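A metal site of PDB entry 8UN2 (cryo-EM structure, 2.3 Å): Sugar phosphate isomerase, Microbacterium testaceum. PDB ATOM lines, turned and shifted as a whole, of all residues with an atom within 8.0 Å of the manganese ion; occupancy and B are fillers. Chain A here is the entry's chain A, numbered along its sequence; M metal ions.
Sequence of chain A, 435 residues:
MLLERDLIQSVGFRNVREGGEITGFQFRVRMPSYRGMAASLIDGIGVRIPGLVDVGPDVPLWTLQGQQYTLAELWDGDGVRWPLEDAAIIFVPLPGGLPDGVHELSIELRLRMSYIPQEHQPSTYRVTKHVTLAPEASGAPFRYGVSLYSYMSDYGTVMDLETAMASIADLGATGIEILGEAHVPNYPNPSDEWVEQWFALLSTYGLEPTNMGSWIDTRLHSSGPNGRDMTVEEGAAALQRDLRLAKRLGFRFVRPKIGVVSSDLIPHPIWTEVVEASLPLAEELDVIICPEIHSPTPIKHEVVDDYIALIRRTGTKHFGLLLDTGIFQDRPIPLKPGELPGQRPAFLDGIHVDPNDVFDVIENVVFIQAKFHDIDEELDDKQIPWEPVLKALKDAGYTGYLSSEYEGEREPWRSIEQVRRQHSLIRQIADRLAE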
ATOM      1  N   SER A 147      19.032  12.375   3.894  1.00  0.00           N
ATOM      2  CA  SER A 147      19.404  11.350   2.930  1.00  0.00           C
ATOM      3  C   SER A 147      19.409  11.949   1.530  1.00  0.00           C
ATOM      4  O   SER A 147      18.544  12.742   1.180  1.00  0.00           O
ATOM      5  CB  SER A 147      18.442  10.169   2.980  1.00  0.00           C
ATOM      6  OG  SER A 147      18.530   9.423   1.798  1.00  0.00           O
ATOM      7  N   TYR A 149      18.641  10.404  -1.046  1.00  0.00           N
ATOM      8  CA  TYR A 149      17.468   9.898  -1.740  1.00  0.00           C
ATOM      9  C   TYR A 149      16.365  10.941  -1.810  1.00  0.00           C
ATOM     10  O   TYR A 149      15.501  10.850  -2.698  1.00  0.00           O
ATOM     11  CB  TYR A 149      16.992   8.626  -1.036  1.00  0.00           C
ATOM     12  CG  TYR A 149      15.667   8.105  -1.500  1.00  0.00           C
ATOM     13  CD1 TYR A 149      15.529   7.467  -2.715  1.00  0.00           C
ATOM     14  CD2 TYR A 149      14.534   8.275  -0.722  1.00  0.00           C
ATOM     15  CE1 TYR A 149      14.318   7.007  -3.141  1.00  0.00           C
ATOM     16  CE2 TYR A 149      13.324   7.814  -1.148  1.00  0.00           C
ATOM     17  CZ  TYR A 149      13.215   7.179  -2.351  1.00  0.00           C
ATOM     18  OH  TYR A 149      11.995   6.719  -2.779  1.00  0.00           O
ATOM     19  N   GLU A 177      23.277  10.816   4.469  1.00  0.00           N
ATOM     20  CA  GLU A 177      23.031   9.432   4.124  1.00  0.00           C
ATOM     21  C   GLU A 177      22.982   9.311   2.616  1.00  0.00           C
ATOM     22  O   GLU A 177      22.331  10.112   1.949  1.00  0.00           O
ATOM     23  CB  GLU A 177      21.735   8.933   4.744  1.00  0.00           C
ATOM     24  CG  GLU A 177      21.112   7.759   4.043  1.00  0.00           C
ATOM     25  CD  GLU A 177      19.862   7.273   4.716  1.00  0.00           C
ATOM     26  OE1 GLU A 177      19.327   8.004   5.564  1.00  0.00           O
ATOM     27  OE2 GLU A 177      19.420   6.154   4.405  1.00  0.00           O
ATOM     28  N   LEU A 179      22.814   6.467  -0.904  1.00  0.00           N
ATOM     29  CA  LEU A 179      22.710   5.130  -1.451  1.00  0.00           C
ATOM     30  C   LEU A 179      23.975   4.863  -2.244  1.00  0.00           C
ATOM     31  O   LEU A 179      24.284   5.599  -3.182  1.00  0.00           O
ATOM     32  CB  LEU A 179      21.485   4.987  -2.346  1.00  0.00           C
ATOM     33  CG  LEU A 179      20.172   5.563  -1.838  1.00  0.00           C
ATOM     34  CD1 LEU A 179      19.240   5.809  -2.994  1.00  0.00           C
ATOM     35  CD2 LEU A 179      19.536   4.613  -0.849  1.00  0.00           C
ATOM     36  N   ARG A 255      22.545  -0.399   5.187  1.00  0.00           N
ATOM     37  CA  ARG A 255      21.194  -0.921   5.091  1.00  0.00           C
ATOM     38  C   ARG A 255      21.082  -1.833   3.888  1.00  0.00           C
ATOM     39  O   ARG A 255      21.002  -1.323   2.756  1.00  0.00           O
ATOM     40  CB  ARG A 255      20.186   0.212   5.003  1.00  0.00           C
ATOM     41  CG  ARG A 255      18.751  -0.239   4.917  1.00  0.00           C
ATOM     42  CD  ARG A 255      18.013   0.485   3.819  1.00  0.00           C
ATOM     43  NE  ARG A 255      18.482   0.074   2.510  1.00  0.00           N
ATOM     44  CZ  ARG A 255      18.095   0.638   1.365  1.00  0.00           C
ATOM     45  NH1 ARG A 255      17.229   1.631   1.386  1.00  0.00           N
ATOM     46  NH2 ARG A 255      18.571   0.197   0.219  1.00  0.00           N
ATOM     47  N   LYS A 257      19.048  -4.168   1.333  1.00  0.00           N
ATOM     48  CA  LYS A 257      17.676  -4.391   0.889  1.00  0.00           C
ATOM     49  C   LYS A 257      17.638  -5.720   0.149  1.00  0.00           C
ATOM     50  O   LYS A 257      18.039  -5.794  -1.012  1.00  0.00           O
ATOM     51  CB  LYS A 257      17.205  -3.240   0.016  1.00  0.00           C
ATOM     52  CG  LYS A 257      15.786  -3.379  -0.462  1.00  0.00           C
ATOM     53  CD  LYS A 257      14.803  -3.274   0.676  1.00  0.00           C
ATOM     54  CE  LYS A 257      14.564  -1.845   1.052  1.00  0.00           C
ATOM     55  NZ  LYS A 257      13.832  -1.133  -0.026  1.00  0.00           N
ATOM     56  N   GLU A 292      15.865  -2.326   6.809  1.00  0.00           N
ATOM     57  CA  GLU A 292      14.851  -1.286   6.912  1.00  0.00           C
ATOM     58  C   GLU A 292      13.495  -1.875   7.276  1.00  0.00           C
ATOM     59  O   GLU A 292      13.089  -2.920   6.753  1.00  0.00           O
ATOM     60  CB  GLU A 292      14.763  -0.536   5.589  1.00  0.00           C
ATOM     61  CG  GLU A 292      13.919   0.712   5.601  1.00  0.00           C
ATOM     62  CD  GLU A 292      13.833   1.344   4.224  1.00  0.00           C
ATOM     63  OE1 GLU A 292      14.209   0.670   3.247  1.00  0.00           O
ATOM     64  OE2 GLU A 292      13.397   2.499   4.124  1.00  0.00           O
ATOM     65  N   ILE A 293      12.803  -1.202   8.191  1.00  0.00           N
ATOM     66  CA  ILE A 293      11.427  -1.534   8.555  1.00  0.00           C
ATOM     67  C   ILE A 293      10.537  -0.464   7.953  1.00  0.00           C
ATOM     68  O   ILE A 293      10.408   0.627   8.493  1.00  0.00           O
ATOM     69  CB  ILE A 293      11.258  -1.600  10.080  1.00  0.00           C
ATOM     70  CG1 ILE A 293      12.238  -2.595  10.697  1.00  0.00           C
ATOM     71  CG2 ILE A 293       9.837  -1.992  10.432  1.00  0.00           C
ATOM     72  CD1 ILE A 293      12.201  -3.958  10.074  1.00  0.00           C
ATOM     73  N   HIS A 294       9.909  -0.783   6.819  1.00  0.00           N
ATOM     74  CA  HIS A 294       9.160   0.208   6.061  1.00  0.00           C
ATOM     75  C   HIS A 294       7.808  -0.380   5.673  1.00  0.00           C
ATOM     76  O   HIS A 294       7.612  -1.594   5.650  1.00  0.00           O
ATOM     77  CB  HIS A 294       9.920   0.647   4.800  1.00  0.00           C
ATOM     78  CG  HIS A 294      10.162  -0.458   3.821  1.00  0.00           C
ATOM     79  ND1 HIS A 294       9.644  -0.443   2.548  1.00  0.00           N
ATOM     80  CD2 HIS A 294      10.871  -1.612   3.933  1.00  0.00           C
ATOM     81  CE1 HIS A 294      10.017  -1.535   1.913  1.00  0.00           C
ATOM     82  NE2 HIS A 294      10.761  -2.261   2.727  1.00  0.00           N
ATOM     83  N   SER A 295       6.880   0.526   5.367  1.00  0.00           N
ATOM     84  CA  SER A 295       5.519   0.156   5.017  1.00  0.00           C
ATOM     85  C   SER A 295       5.505  -0.633   3.716  1.00  0.00           C
ATOM     86  O   SER A 295       6.278  -0.311   2.805  1.00  0.00           O
ATOM     87  CB  SER A 295       4.684   1.421   4.888  1.00  0.00           C
ATOM     88  OG  SER A 295       3.345   1.152   4.534  1.00  0.00           O
ATOM     89  N   LEU A 322      16.559  -0.346  11.365  1.00  0.00           N
ATOM     90  CA  LEU A 322      16.314   0.966  10.780  1.00  0.00           C
ATOM     91  C   LEU A 322      14.815   1.178  10.715  1.00  0.00           C
ATOM     92  O   LEU A 322      14.092   0.310  10.218  1.00  0.00           O
ATOM     93  CB  LEU A 322      16.946   1.065   9.399  1.00  0.00           C
ATOM     94  CG  LEU A 322      17.189   2.438   8.798  1.00  0.00           C
ATOM     95  CD1 LEU A 322      18.470   2.436   8.049  1.00  0.00           C
ATOM     96  CD2 LEU A 322      16.068   2.786   7.877  1.00  0.00           C
ATOM     97  N   LEU A 323      14.355   2.313  11.200  1.00  0.00           N
ATOM     98  CA  LEU A 323      12.940   2.604  11.267  1.00  0.00           C
ATOM     99  C   LEU A 323      12.569   3.652  10.227  1.00  0.00           C
ATOM    100  O   LEU A 323      13.109   4.759  10.228  1.00  0.00           O
ATOM    101  CB  LEU A 323      12.561   3.097  12.658  1.00  0.00           C
ATOM    102  CG  LEU A 323      11.145   2.795  13.133  1.00  0.00           C
ATOM    103  CD1 LEU A 323      10.972   1.315  13.246  1.00  0.00           C
ATOM    104  CD2 LEU A 323      10.907   3.462  14.465  1.00  0.00           C
ATOM    105  N   ASP A 324      11.662   3.296   9.342  1.00  0.00           N
ATOM    106  CA  ASP A 324      11.137   4.229   8.357  1.00  0.00           C
ATOM    107  C   ASP A 324       9.797   4.744   8.855  1.00  0.00           C
ATOM    108  O   ASP A 324       8.903   3.959   9.153  1.00  0.00           O
ATOM    109  CB  ASP A 324      10.992   3.552   7.001  1.00  0.00           C
ATOM    110  CG  ASP A 324      10.827   4.530   5.860  1.00  0.00           C
ATOM    111  OD1 ASP A 324      11.811   4.770   5.132  1.00  0.00           O
ATOM    112  OD2 ASP A 324       9.714   5.033   5.674  1.00  0.00           O
ATOM    113  N   THR A 325       9.662   6.073   8.955  1.00  0.00           N
ATOM    114  CA  THR A 325       8.465   6.667   9.528  1.00  0.00           C
ATOM    115  C   THR A 325       7.276   6.692   8.586  1.00  0.00           C
ATOM    116  O   THR A 325       6.267   7.331   8.912  1.00  0.00           O
ATOM    117  CB  THR A 325       8.741   8.092  10.002  1.00  0.00           C
ATOM    118  OG1 THR A 325       8.876   8.959   8.877  1.00  0.00           O
ATOM    119  CG2 THR A 325       9.994   8.152  10.833  1.00  0.00           C
ATOM    120  N   GLY A 326       7.349   6.019   7.439  1.00  0.00           N
ATOM    121  CA  GLY A 326       6.165   5.859   6.606  1.00  0.00           C
ATOM    122  C   GLY A 326       5.171   4.876   7.183  1.00  0.00           C
ATOM    123  O   GLY A 326       4.024   4.830   6.729  1.00  0.00           O
ATOM    124  N   ILE A 368      16.875   6.263  12.007  1.00  0.00           N
ATOM    125  CA  ILE A 368      15.503   6.522  11.621  1.00  0.00           C
ATOM    126  C   ILE A 368      15.480   7.375  10.365  1.00  0.00           C
ATOM    127  O   ILE A 368      16.081   8.452  10.341  1.00  0.00           O
ATOM    128  CB  ILE A 368      14.701   7.186  12.750  1.00  0.00           C
ATOM    129  CG1 ILE A 368      14.410   6.178  13.852  1.00  0.00           C
ATOM    130  CG2 ILE A 368      13.400   7.722  12.236  1.00  0.00           C
ATOM    131  CD1 ILE A 368      13.635   6.730  14.984  1.00  0.00           C
ATOM    132  N   GLN A 369      14.820   6.884   9.329  1.00  0.00           N
ATOM    133  CA  GLN A 369      14.598   7.639   8.104  1.00  0.00           C
ATOM    134  C   GLN A 369      13.283   8.395   8.233  1.00  0.00           C
ATOM    135  O   GLN A 369      12.214   7.781   8.233  1.00  0.00           O
ATOM    136  CB  GLN A 369      14.566   6.713   6.902  1.00  0.00           C
ATOM    137  CG  GLN A 369      15.915   6.294   6.425  1.00  0.00           C
ATOM    138  CD  GLN A 369      15.840   5.240   5.351  1.00  0.00           C
ATOM    139  OE1 GLN A 369      14.766   4.919   4.865  1.00  0.00           O
ATOM    140  NE2 GLN A 369      16.985   4.684   4.990  1.00  0.00           N
ATOM    141  N   ALA A 370      13.368   9.715   8.349  1.00  0.00           N
ATOM    142  CA  ALA A 370      12.185  10.553   8.479  1.00  0.00           C
ATOM    143  C   ALA A 370      11.519  10.683   7.113  1.00  0.00           C
ATOM    144  O   ALA A 370      11.866  11.556   6.327  1.00  0.00           O
ATOM    145  CB  ALA A 370      12.562  11.910   9.050  1.00  0.00           C
ATOM    146  N   LYS A 371      10.563   9.805   6.848  1.00  0.00           N
ATOM    147  CA  LYS A 371       9.882   9.728   5.567  1.00  0.00           C
ATOM    148  C   LYS A 371       8.697  10.676   5.567  1.00  0.00           C
ATOM    149  O   LYS A 371       7.933  10.720   6.527  1.00  0.00           O
ATOM    150  CB  LYS A 371       9.403   8.299   5.324  1.00  0.00           C
ATOM    151  CG  LYS A 371       8.568   8.094   4.095  1.00  0.00           C
ATOM    152  CD  LYS A 371       9.422   8.007   2.869  1.00  0.00           C
ATOM    153  CE  LYS A 371      10.253   6.749   2.875  1.00  0.00           C
ATOM    154  NZ  LYS A 371       9.406   5.539   2.878  1.00  0.00           N
ATOM    155  N   SER A 403      17.096  11.159   9.569  1.00  0.00           N
ATOM    156  CA  SER A 403      17.474  11.532   8.214  1.00  0.00           C
ATOM    157  C   SER A 403      16.227  11.765   7.374  1.00  0.00           C
ATOM    158  O   SER A 403      15.325  10.928   7.360  1.00  0.00           O
ATOM    159  CB  SER A 403      18.352  10.483   7.563  1.00  0.00           C
ATOM    160  OG  SER A 403      19.699  10.675   7.931  1.00  0.00           O
ATOM    161  N   GLU A 405      13.838  11.783   4.342  1.00  0.00           N
ATOM    162  CA  GLU A 405      13.589  11.045   3.104  1.00  0.00           C
ATOM    163  C   GLU A 405      12.338  11.606   2.456  1.00  0.00           C
ATOM    164  O   GLU A 405      11.215  11.307   2.859  1.00  0.00           O
ATOM    165  CB  GLU A 405      13.458   9.559   3.355  1.00  0.00           C
ATOM    166  CG  GLU A 405      14.789   8.870   3.410  1.00  0.00           C
ATOM    167  CD  GLU A 405      14.707   7.444   2.921  1.00  0.00           C
ATOM    168  OE1 GLU A 405      13.586   6.913   2.770  1.00  0.00           O
ATOM    169  OE2 GLU A 405      15.774   6.850   2.664  1.00  0.00           O
ATOM    170  N   GLU A 407       9.611  11.781  -0.323  1.00  0.00           N
ATOM    171  CA  GLU A 407       8.989  10.749  -1.139  1.00  0.00           C
ATOM    172  C   GLU A 407       7.915  11.354  -2.021  1.00  0.00           C
ATOM    173  O   GLU A 407       7.188  10.645  -2.741  1.00  0.00           O
ATOM    174  CB  GLU A 407       8.419   9.660  -0.235  1.00  0.00           C
ATOM    175  CG  GLU A 407       8.089   8.309  -0.856  1.00  0.00           C
ATOM    176  CD  GLU A 407       9.298   7.516  -1.228  1.00  0.00           C
ATOM    177  OE1 GLU A 407      10.260   7.537  -0.457  1.00  0.00           O
ATOM    178  OE2 GLU A 407       9.282   6.863  -2.296  1.00  0.00           O
HETATM  179 MN    MN M   1      13.212   4.389   3.466  1.00  0.00          MN
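NZ of Lys 371 is in salt-bridge range of OE1 of Glu 407 (3.98 Å).
The side-chain carboxylate of Glu 292 is in salt-bridge range of the side-chain amino group of Lys 257, 3.8 Å away.
O of Gln 369 is in hydrogen-bond range of N of Thr 325.
N of Gln 369 lies within hydrogen-bond range of O of Leu 323, at 2.9 Å.
The side-chain carboxylate of Glu 177 sits at hydrogen-bond distance from the side-chain amide nitrogen of Gln 369, at 2.9 Å.
The backbone NH of Gly 326 sits close to the side-chain carboxylate of Asp 324 (3.1 Å).
NH1 of Arg 255 lies within salt-bridge range of OE1 of Glu 292 (3.7 Å).
The backbone NH of Glu 405 is in hydrogen-bond range of the backbone carbonyl oxygen of Ala 370 (2.8 Å).
Merely in contact with the manganese ion: Lys 371 (3.8 Å).
Five residues have an atom within 4 Å of the manganese ion: Glu 292, Asp 324, Gln 369, Lys 371 and Glu 405.
The nearest printed residue that does not touch the manganese ion is His 294 (5.2 Å).
The manganese ion is bound by OE2 of Glu 292, OE1 of Gln 369, OD1 of Asp 324 and OE1 of Glu 405.
The manganese ion has four donor atoms within binding distance.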
